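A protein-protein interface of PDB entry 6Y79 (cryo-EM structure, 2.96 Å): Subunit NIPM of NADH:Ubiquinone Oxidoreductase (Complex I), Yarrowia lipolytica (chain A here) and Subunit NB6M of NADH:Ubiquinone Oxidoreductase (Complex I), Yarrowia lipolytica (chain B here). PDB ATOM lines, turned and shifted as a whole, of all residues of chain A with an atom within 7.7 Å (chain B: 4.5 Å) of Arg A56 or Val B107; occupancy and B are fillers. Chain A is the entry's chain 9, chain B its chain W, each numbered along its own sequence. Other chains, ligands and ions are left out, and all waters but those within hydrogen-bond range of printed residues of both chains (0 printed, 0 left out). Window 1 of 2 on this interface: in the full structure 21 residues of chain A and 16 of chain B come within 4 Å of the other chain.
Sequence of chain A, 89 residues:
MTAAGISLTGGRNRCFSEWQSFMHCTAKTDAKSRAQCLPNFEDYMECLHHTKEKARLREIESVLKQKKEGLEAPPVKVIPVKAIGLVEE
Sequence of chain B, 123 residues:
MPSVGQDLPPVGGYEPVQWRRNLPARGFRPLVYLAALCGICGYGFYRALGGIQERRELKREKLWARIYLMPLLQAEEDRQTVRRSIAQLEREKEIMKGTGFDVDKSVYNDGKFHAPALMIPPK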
ATOM      1  N   GLU A  42      -4.276  -4.156  25.392  1.00  0.00           N
ATOM      2  CA  GLU A  42      -3.053  -4.644  24.768  1.00  0.00           C
ATOM      3  C   GLU A  42      -2.919  -4.090  23.361  1.00  0.00           C
ATOM      4  O   GLU A  42      -1.858  -3.563  22.999  1.00  0.00           O
ATOM      5  CB  GLU A  42      -3.040  -6.169  24.753  1.00  0.00           C
ATOM      6  CG  GLU A  42      -2.757  -6.805  26.097  1.00  0.00           C
ATOM      7  CD  GLU A  42      -2.959  -8.307  26.081  1.00  0.00           C
ATOM      8  OE1 GLU A  42      -3.414  -8.833  25.046  1.00  0.00           O
ATOM      9  OE2 GLU A  42      -2.667  -8.960  27.105  1.00  0.00           O
ATOM     10  N   ASP A  43      -4.037  -4.077  22.620  1.00  0.00           N
ATOM     11  CA  ASP A  43      -4.067  -3.498  21.282  1.00  0.00           C
ATOM     12  C   ASP A  43      -3.746  -2.019  21.314  1.00  0.00           C
ATOM     13  O   ASP A  43      -3.153  -1.486  20.372  1.00  0.00           O
ATOM     14  CB  ASP A  43      -5.437  -3.705  20.650  1.00  0.00           C
ATOM     15  CG  ASP A  43      -5.717  -5.141  20.364  1.00  0.00           C
ATOM     16  OD1 ASP A  43      -4.759  -5.933  20.436  1.00  0.00           O
ATOM     17  OD2 ASP A  43      -6.883  -5.475  20.067  1.00  0.00           O
ATOM     18  N   GLU A  46       0.453  -1.680  22.397  1.00  0.00           N
ATOM     19  CA  GLU A  46       1.365  -1.927  21.307  1.00  0.00           C
ATOM     20  C   GLU A  46       1.013  -1.102  20.066  1.00  0.00           C
ATOM     21  O   GLU A  46       1.863  -0.964  19.186  1.00  0.00           O
ATOM     22  CB  GLU A  46       1.435  -3.442  21.086  1.00  0.00           C
ATOM     23  CG  GLU A  46       2.498  -3.914  20.183  1.00  0.00           C
ATOM     24  CD  GLU A  46       1.934  -4.060  18.795  1.00  0.00           C
ATOM     25  OE1 GLU A  46       0.768  -4.484  18.747  1.00  0.00           O
ATOM     26  OE2 GLU A  46       2.621  -3.747  17.834  1.00  0.00           O
ATOM     27  N   CYS A  47      -0.171  -0.468  20.008  1.00  0.00           N
ATOM     28  CA  CYS A  47      -0.339   0.638  19.067  1.00  0.00           C
ATOM     29  C   CYS A  47       0.628   1.758  19.390  1.00  0.00           C
ATOM     30  O   CYS A  47       1.193   2.377  18.487  1.00  0.00           O
ATOM     31  CB  CYS A  47      -1.760   1.197  19.089  1.00  0.00           C
ATOM     32  SG  CYS A  47      -2.055   2.579  17.905  1.00  0.00           S
ATOM     33  N   HIS A  50       4.699  -0.328  19.728  1.00  0.00           N
ATOM     34  CA  HIS A  50       5.078  -1.313  18.705  1.00  0.00           C
ATOM     35  C   HIS A  50       6.022  -2.377  19.260  1.00  0.00           C
ATOM     36  O   HIS A  50       7.028  -2.716  18.643  1.00  0.00           O
ATOM     37  CB  HIS A  50       5.686  -0.642  17.470  1.00  0.00           C
ATOM     38  CG  HIS A  50       4.753   0.280  16.755  1.00  0.00           C
ATOM     39  ND1 HIS A  50       3.619  -0.162  16.113  1.00  0.00           N
ATOM     40  CD2 HIS A  50       4.798   1.618  16.564  1.00  0.00           C
ATOM     41  CE1 HIS A  50       2.997   0.867  15.567  1.00  0.00           C
ATOM     42  NE2 HIS A  50       3.692   1.958  15.826  1.00  0.00           N
ATOM     43  N   THR A  51       5.701  -2.889  20.445  1.00  0.00           N
ATOM     44  CA  THR A  51       6.588  -3.832  21.120  1.00  0.00           C
ATOM     45  C   THR A  51       6.547  -5.201  20.451  1.00  0.00           C
ATOM     46  O   THR A  51       7.593  -5.796  20.155  1.00  0.00           O
ATOM     47  CB  THR A  51       6.204  -3.926  22.597  1.00  0.00           C
ATOM     48  OG1 THR A  51       6.414  -2.655  23.223  1.00  0.00           O
ATOM     49  CG2 THR A  51       7.037  -4.965  23.306  1.00  0.00           C
ATOM     50  N   LYS A  52       5.344  -5.703  20.180  1.00  0.00           N
ATOM     51  CA  LYS A  52       5.214  -7.015  19.566  1.00  0.00           C
ATOM     52  C   LYS A  52       5.648  -7.012  18.103  1.00  0.00           C
ATOM     53  O   LYS A  52       6.158  -8.026  17.621  1.00  0.00           O
ATOM     54  CB  LYS A  52       3.782  -7.523  19.719  1.00  0.00           C
ATOM     55  CG  LYS A  52       3.400  -7.838  21.158  1.00  0.00           C
ATOM     56  CD  LYS A  52       1.948  -8.252  21.270  1.00  0.00           C
ATOM     57  CE  LYS A  52       1.605  -8.670  22.687  1.00  0.00           C
ATOM     58  NZ  LYS A  52       0.174  -9.047  22.823  1.00  0.00           N
ATOM     59  N   GLU A  53       5.504  -5.890  17.393  1.00  0.00           N
ATOM     60  CA  GLU A  53       6.000  -5.833  16.020  1.00  0.00           C
ATOM     61  C   GLU A  53       7.515  -5.759  15.981  1.00  0.00           C
ATOM     62  O   GLU A  53       8.136  -6.332  15.087  1.00  0.00           O
ATOM     63  CB  GLU A  53       5.398  -4.654  15.256  1.00  0.00           C
ATOM     64  CG  GLU A  53       3.995  -4.967  14.856  1.00  0.00           C
ATOM     65  CD  GLU A  53       3.585  -4.655  13.437  1.00  0.00           C
ATOM     66  OE1 GLU A  53       3.181  -3.506  13.167  1.00  0.00           O
ATOM     67  OE2 GLU A  53       3.650  -5.570  12.585  1.00  0.00           O
ATOM     68  N   LYS A  54       8.129  -5.068  16.947  1.00  0.00           N
ATOM     69  CA  LYS A  54       9.584  -5.076  17.031  1.00  0.00           C
ATOM     70  C   LYS A  54      10.104  -6.468  17.360  1.00  0.00           C
ATOM     71  O   LYS A  54      11.124  -6.902  16.808  1.00  0.00           O
ATOM     72  CB  LYS A  54      10.051  -4.072  18.072  1.00  0.00           C
ATOM     73  CG  LYS A  54      10.159  -2.652  17.573  1.00  0.00           C
ATOM     74  CD  LYS A  54      10.561  -1.705  18.682  1.00  0.00           C
ATOM     75  CE  LYS A  54      10.425  -0.261  18.252  1.00  0.00           C
ATOM     76  NZ  LYS A  54      10.920   0.666  19.299  1.00  0.00           N
ATOM     77  N   ALA A  55       9.390  -7.196  18.225  1.00  0.00           N
ATOM     78  CA  ALA A  55       9.771  -8.570  18.545  1.00  0.00           C
ATOM     79  C   ALA A  55       9.640  -9.481  17.329  1.00  0.00           C
ATOM     80  O   ALA A  55      10.537 -10.287  17.041  1.00  0.00           O
ATOM     81  CB  ALA A  55       8.917  -9.088  19.700  1.00  0.00           C
ATOM     82  N   ARG A  56       8.531  -9.350  16.593  1.00  0.00           N
ATOM     83  CA  ARG A  56       8.309 -10.165  15.402  1.00  0.00           C
ATOM     84  C   ARG A  56       9.337  -9.869  14.318  1.00  0.00           C
ATOM     85  O   ARG A  56       9.896 -10.793  13.719  1.00  0.00           O
ATOM     86  CB  ARG A  56       6.894  -9.934  14.881  1.00  0.00           C
ATOM     87  CG  ARG A  56       6.487 -10.765  13.682  1.00  0.00           C
ATOM     88  CD  ARG A  56       5.011 -10.519  13.400  1.00  0.00           C
ATOM     89  NE  ARG A  56       4.501 -11.199  12.217  1.00  0.00           N
ATOM     90  CZ  ARG A  56       4.605 -10.716  10.984  1.00  0.00           C
ATOM     91  NH1 ARG A  56       5.216  -9.563  10.771  1.00  0.00           N
ATOM     92  NH2 ARG A  56       4.105 -11.386   9.959  1.00  0.00           N
ATOM     93  N   LEU A  57       9.646  -8.594  14.093  1.00  0.00           N
ATOM     94  CA  LEU A  57      10.611  -8.255  13.056  1.00  0.00           C
ATOM     95  C   LEU A  57      12.030  -8.632  13.454  1.00  0.00           C
ATOM     96  O   LEU A  57      12.840  -8.967  12.583  1.00  0.00           O
ATOM     97  CB  LEU A  57      10.502  -6.774  12.713  1.00  0.00           C
ATOM     98  CG  LEU A  57       9.152  -6.510  12.043  1.00  0.00           C
ATOM     99  CD1 LEU A  57       8.754  -5.059  12.136  1.00  0.00           C
ATOM    100  CD2 LEU A  57       9.150  -6.966  10.615  1.00  0.00           C
ATOM    101  N   ARG A  58      12.342  -8.653  14.754  1.00  0.00           N
ATOM    102  CA  ARG A  58      13.635  -9.195  15.152  1.00  0.00           C
ATOM    103  C   ARG A  58      13.702 -10.700  14.946  1.00  0.00           C
ATOM    104  O   ARG A  58      14.746 -11.215  14.521  1.00  0.00           O
ATOM    105  CB  ARG A  58      13.948  -8.839  16.604  1.00  0.00           C
ATOM    106  CG  ARG A  58      15.420  -9.026  16.938  1.00  0.00           C
ATOM    107  CD  ARG A  58      15.789  -8.472  18.295  1.00  0.00           C
ATOM    108  NE  ARG A  58      15.803  -7.014  18.305  1.00  0.00           N
ATOM    109  CZ  ARG A  58      16.868  -6.275  18.014  1.00  0.00           C
ATOM    110  NH1 ARG A  58      16.788  -4.953  18.052  1.00  0.00           N
ATOM    111  NH2 ARG A  58      18.013  -6.859  17.681  1.00  0.00           N
ATOM    112  N   GLU A  59      12.587 -11.399  15.191  1.00  0.00           N
ATOM    113  CA  GLU A  59      12.525 -12.836  14.944  1.00  0.00           C
ATOM    114  C   GLU A  59      12.694 -13.173  13.463  1.00  0.00           C
ATOM    115  O   GLU A  59      13.329 -14.179  13.130  1.00  0.00           O
ATOM    116  CB  GLU A  59      11.206 -13.392  15.485  1.00  0.00           C
ATOM    117  CG  GLU A  59      11.010 -14.887  15.304  1.00  0.00           C
ATOM    118  CD  GLU A  59      10.381 -15.555  16.514  1.00  0.00           C
ATOM    119  OE1 GLU A  59       9.858 -16.681  16.370  1.00  0.00           O
ATOM    120  OE2 GLU A  59      10.416 -14.962  17.613  1.00  0.00           O
ATOM    121  N   ILE A  60      12.173 -12.343  12.560  1.00  0.00           N
ATOM    122  CA  ILE A  60      12.341 -12.645  11.135  1.00  0.00           C
ATOM    123  C   ILE A  60      13.708 -12.182  10.605  1.00  0.00           C
ATOM    124  O   ILE A  60      14.247 -12.786   9.664  1.00  0.00           O
ATOM    125  CB  ILE A  60      11.182 -12.064  10.292  1.00  0.00           C
ATOM    126  CG1 ILE A  60      11.291 -10.561  10.097  1.00  0.00           C
ATOM    127  CG2 ILE A  60       9.838 -12.342  10.923  1.00  0.00           C
ATOM    128  CD1 ILE A  60      10.376 -10.077   9.039  1.00  0.00           C
ATOM    129  N   GLU A  61      14.300 -11.139  11.202  1.00  0.00           N
ATOM    130  CA  GLU A  61      15.593 -10.655  10.734  1.00  0.00           C
ATOM    131  C   GLU A  61      16.711 -11.567  11.204  1.00  0.00           C
ATOM    132  O   GLU A  61      17.717 -11.725  10.495  1.00  0.00           O
ATOM    133  CB  GLU A  61      15.805  -9.214  11.212  1.00  0.00           C
ATOM    134  CG  GLU A  61      16.881  -8.391  10.502  1.00  0.00           C
ATOM    135  CD  GLU A  61      18.213  -8.467  11.192  1.00  0.00           C
ATOM    136  OE1 GLU A  61      18.224  -8.825  12.380  1.00  0.00           O
ATOM    137  OE2 GLU A  61      19.261  -8.097  10.582  1.00  0.00           O
ATOM    138  N   SER A  62      16.511 -12.224  12.363  1.00  0.00           N
ATOM    139  CA  SER A  62      17.419 -13.268  12.840  1.00  0.00           C
ATOM    140  C   SER A  62      17.524 -14.433  11.859  1.00  0.00           C
ATOM    141  O   SER A  62      18.579 -15.077  11.771  1.00  0.00           O
ATOM    142  CB  SER A  62      16.950 -13.782  14.210  1.00  0.00           C
ATOM    143  OG  SER A  62      15.841 -14.669  14.110  1.00  0.00           O
ATOM    144  N   GLU B  92       7.880 -12.087   3.439  1.00  0.00           N
ATOM    145  CA  GLU B  92       8.446 -12.729   4.625  1.00  0.00           C
ATOM    146  C   GLU B  92       7.931 -14.156   4.804  1.00  0.00           C
ATOM    147  O   GLU B  92       8.535 -14.929   5.556  1.00  0.00           O
ATOM    148  CB  GLU B  92       8.199 -11.894   5.877  1.00  0.00           C
ATOM    149  CG  GLU B  92       6.791 -11.415   6.099  1.00  0.00           C
ATOM    150  CD  GLU B  92       6.771 -10.102   6.852  1.00  0.00           C
ATOM    151  OE1 GLU B  92       5.697  -9.691   7.332  1.00  0.00           O
ATOM    152  OE2 GLU B  92       7.843  -9.466   6.951  1.00  0.00           O
ATOM    153  N   PHE B 101       7.114 -20.841  11.552  1.00  0.00           N
ATOM    154  CA  PHE B 101       6.802 -19.526  12.090  1.00  0.00           C
ATOM    155  C   PHE B 101       5.603 -18.980  11.330  1.00  0.00           C
ATOM    156  O   PHE B 101       5.532 -19.102  10.105  1.00  0.00           O
ATOM    157  CB  PHE B 101       7.997 -18.576  11.962  1.00  0.00           C
ATOM    158  CG  PHE B 101       7.745 -17.196  12.502  1.00  0.00           C
ATOM    159  CD1 PHE B 101       7.783 -16.948  13.863  1.00  0.00           C
ATOM    160  CD2 PHE B 101       7.490 -16.142  11.643  1.00  0.00           C
ATOM    161  CE1 PHE B 101       7.562 -15.673  14.353  1.00  0.00           C
ATOM    162  CE2 PHE B 101       7.273 -14.868  12.123  1.00  0.00           C
ATOM    163  CZ  PHE B 101       7.308 -14.635  13.479  1.00  0.00           C
ATOM    164  N   ASP B 102       4.671 -18.377  12.058  1.00  0.00           N
ATOM    165  CA  ASP B 102       3.469 -17.809  11.457  1.00  0.00           C
ATOM    166  C   ASP B 102       3.747 -16.361  11.071  1.00  0.00           C
ATOM    167  O   ASP B 102       3.911 -15.500  11.940  1.00  0.00           O
ATOM    168  CB  ASP B 102       2.293 -17.907  12.423  1.00  0.00           C
ATOM    169  CG  ASP B 102       0.948 -17.741  11.736  1.00  0.00           C
ATOM    170  OD1 ASP B 102       0.899 -17.352  10.550  1.00  0.00           O
ATOM    171  OD2 ASP B 102      -0.075 -18.023  12.390  1.00  0.00           O
ATOM    172  N   VAL B 103       3.796 -16.087   9.766  1.00  0.00           N
ATOM    173  CA  VAL B 103       3.914 -14.697   9.344  1.00  0.00           C
ATOM    174  C   VAL B 103       2.546 -14.085   9.042  1.00  0.00           C
ATOM    175  O   VAL B 103       2.406 -12.856   9.058  1.00  0.00           O
ATOM    176  CB  VAL B 103       4.862 -14.540   8.141  1.00  0.00           C
ATOM    177  CG1 VAL B 103       6.216 -15.168   8.421  1.00  0.00           C
ATOM    178  CG2 VAL B 103       4.249 -15.120   6.886  1.00  0.00           C
ATOM    179  N   LYS B 105      -0.027 -14.278  10.922  1.00  0.00           N
ATOM    180  CA  LYS B 105      -0.681 -13.889  12.161  1.00  0.00           C
ATOM    181  C   LYS B 105      -0.372 -12.440  12.496  1.00  0.00           C
ATOM    182  O   LYS B 105       0.782 -11.994  12.433  1.00  0.00           O
ATOM    183  CB  LYS B 105      -0.256 -14.777  13.334  1.00  0.00           C
ATOM    184  CG  LYS B 105      -1.068 -14.492  14.601  1.00  0.00           C
ATOM    185  CD  LYS B 105      -0.732 -15.438  15.728  1.00  0.00           C
ATOM    186  CE  LYS B 105       0.739 -15.362  16.051  1.00  0.00           C
ATOM    187  NZ  LYS B 105       1.109 -14.088  16.720  1.00  0.00           N
ATOM    188  N   SER B 106      -1.422 -11.710  12.846  1.00  0.00           N
ATOM    189  CA  SER B 106      -1.298 -10.349  13.331  1.00  0.00           C
ATOM    190  C   SER B 106      -0.755 -10.356  14.746  1.00  0.00           C
ATOM    191  O   SER B 106      -1.008 -11.296  15.505  1.00  0.00           O
ATOM    192  CB  SER B 106      -2.645  -9.659  13.321  1.00  0.00           C
ATOM    193  OG  SER B 106      -3.464 -10.246  14.322  1.00  0.00           O
ATOM    194  N   VAL B 107       0.015  -9.319  15.092  1.00  0.00           N
ATOM    195  CA  VAL B 107       0.318  -9.131  16.498  1.00  0.00           C
ATOM    196  C   VAL B 107      -0.807  -8.394  17.205  1.00  0.00           C
ATOM    197  O   VAL B 107      -0.869  -8.424  18.438  1.00  0.00           O
ATOM    198  CB  VAL B 107       1.632  -8.378  16.702  1.00  0.00           C
ATOM    199  CG1 VAL B 107       2.761  -9.036  15.945  1.00  0.00           C
ATOM    200  CG2 VAL B 107       1.472  -6.966  16.300  1.00  0.00           C
ATOM    201  N   TYR B 108      -1.680  -7.708  16.464  1.00  0.00           N
ATOM    202  CA  TYR B 108      -2.833  -7.068  17.072  1.00  0.00           C
ATOM    203  C   TYR B 108      -3.827  -8.156  17.431  1.00  0.00           C
ATOM    204  O   TYR B 108      -3.964  -9.141  16.707  1.00  0.00           O
ATOM    205  CB  TYR B 108      -3.452  -6.049  16.117  1.00  0.00           C
ATOM    206  CG  TYR B 108      -2.667  -4.764  15.898  1.00  0.00           C
ATOM    207  CD1 TYR B 108      -1.773  -4.264  16.839  1.00  0.00           C
ATOM    208  CD2 TYR B 108      -2.823  -4.035  14.710  1.00  0.00           C
ATOM    209  CE1 TYR B 108      -1.081  -3.077  16.593  1.00  0.00           C
ATOM    210  CE2 TYR B 108      -2.122  -2.863  14.487  1.00  0.00           C
ATOM    211  CZ  TYR B 108      -1.249  -2.398  15.450  1.00  0.00           C
ATOM    212  OH  TYR B 108      -0.556  -1.210  15.203  1.00  0.00           O
ATOM    213  N   ASN B 109      -4.510  -8.003  18.563  1.00  0.00           N
ATOM    214  CA  ASN B 109      -5.434  -9.058  18.954  1.00  0.00           C
ATOM    215  C   ASN B 109      -6.765  -8.961  18.232  1.00  0.00           C
ATOM    216  O   ASN B 109      -7.496  -9.951  18.181  1.00  0.00           O
ATOM    217  CB  ASN B 109      -5.653  -9.054  20.465  1.00  0.00           C
ATOM    218  CG  ASN B 109      -4.472  -9.618  21.218  1.00  0.00           C
ATOM    219  OD1 ASN B 109      -3.867 -10.604  20.794  1.00  0.00           O
ATOM    220  ND2 ASN B 109      -4.127  -8.992  22.339  1.00  0.00           N
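NH1 of Arg A56 is in salt-bridge range of OE1 of Glu B92 (3.5 Å). The backbone NH of Asn B109 sits at hydrogen-bond distance from the side-chain carboxylate of Asp A43, 2.8 Å away. The backbone carbonyl oxygen of Val B103 sits at hydrogen-bond distance from the guanidinium group of Arg A56 (2.4 Å). ND2 of Asn B109 lies within hydrogen-bond range of OE1 of Glu A42, at 2.8 Å.
The backbone NH (N) of Lys B105 lies within hydrogen-bond range of the side-chain carboxylate (OD1) of Asp B102, 3.2 Å away. The side-chain hydroxyl (OG) of Ser A62 is in hydrogen-bond range of the backbone carbonyl oxygen (O) of Glu A59. The side-chain hydroxyl of Ser B106 sits at hydrogen-bond distance from the backbone carbonyl oxygen of Tyr B108.
Among the printed residues, pairs that only touch across the chains: Glu A46 with Tyr B108 (3.2 Å), Glu A59 with Phe B101 (3.2 Å), Ile A60 with Glu B92 (3.3 Å), Glu A53 with Val B107 (3.5 Å), Glu A46 with Val B107 (3.6 Å), Arg A56 with Val B107 (3.7 Å), Ile A60 with Phe B101 (3.8 Å), Lys A52 with Val B107 (3.8 Å), Arg A56 with Lys B105 (3.8 Å), Asp A43 with Tyr B108 (3.9 Å) and Arg A56 with Phe B101 (3.96 Å).
Of chain B, only Glu B92 (3.5 Å), Phe B101 (3.96 Å), Val B103 (2.4 Å), Lys B105 (3.8 Å) and Val B107 (3.7 Å) come within 4 Å of Arg A56. Val B107 touches just these residues of chain A: Glu A46, Lys A52, Glu A53 and Arg A56. Printed residues of chain A within 4 Å of Glu B92: Arg A56 and Ile A60. Of the printed residues of chain B, Asp A43 touches Tyr B108 and Asn B109. His A50 touches none of the printed residues of chain B. Leu A57 touches none of the printed residues of chain B. The nearest residue of chain A that does not touch Val B107 is Asp A43 (5.0 Å).
Along chain B the printed residues that touch a printed residue of chain A span positions 92 to 109. Of the 17 printed residues of chain A, 8 touch a printed residue of chain B. Among the printed residues, 15 pairs touch across the chains. Among the printed residues, Asp or Glu carboxylates within 4 Å of a Lys or Arg side-chain nitrogen of the other chain: Arg A56 with Glu B92 (3.5 Å).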
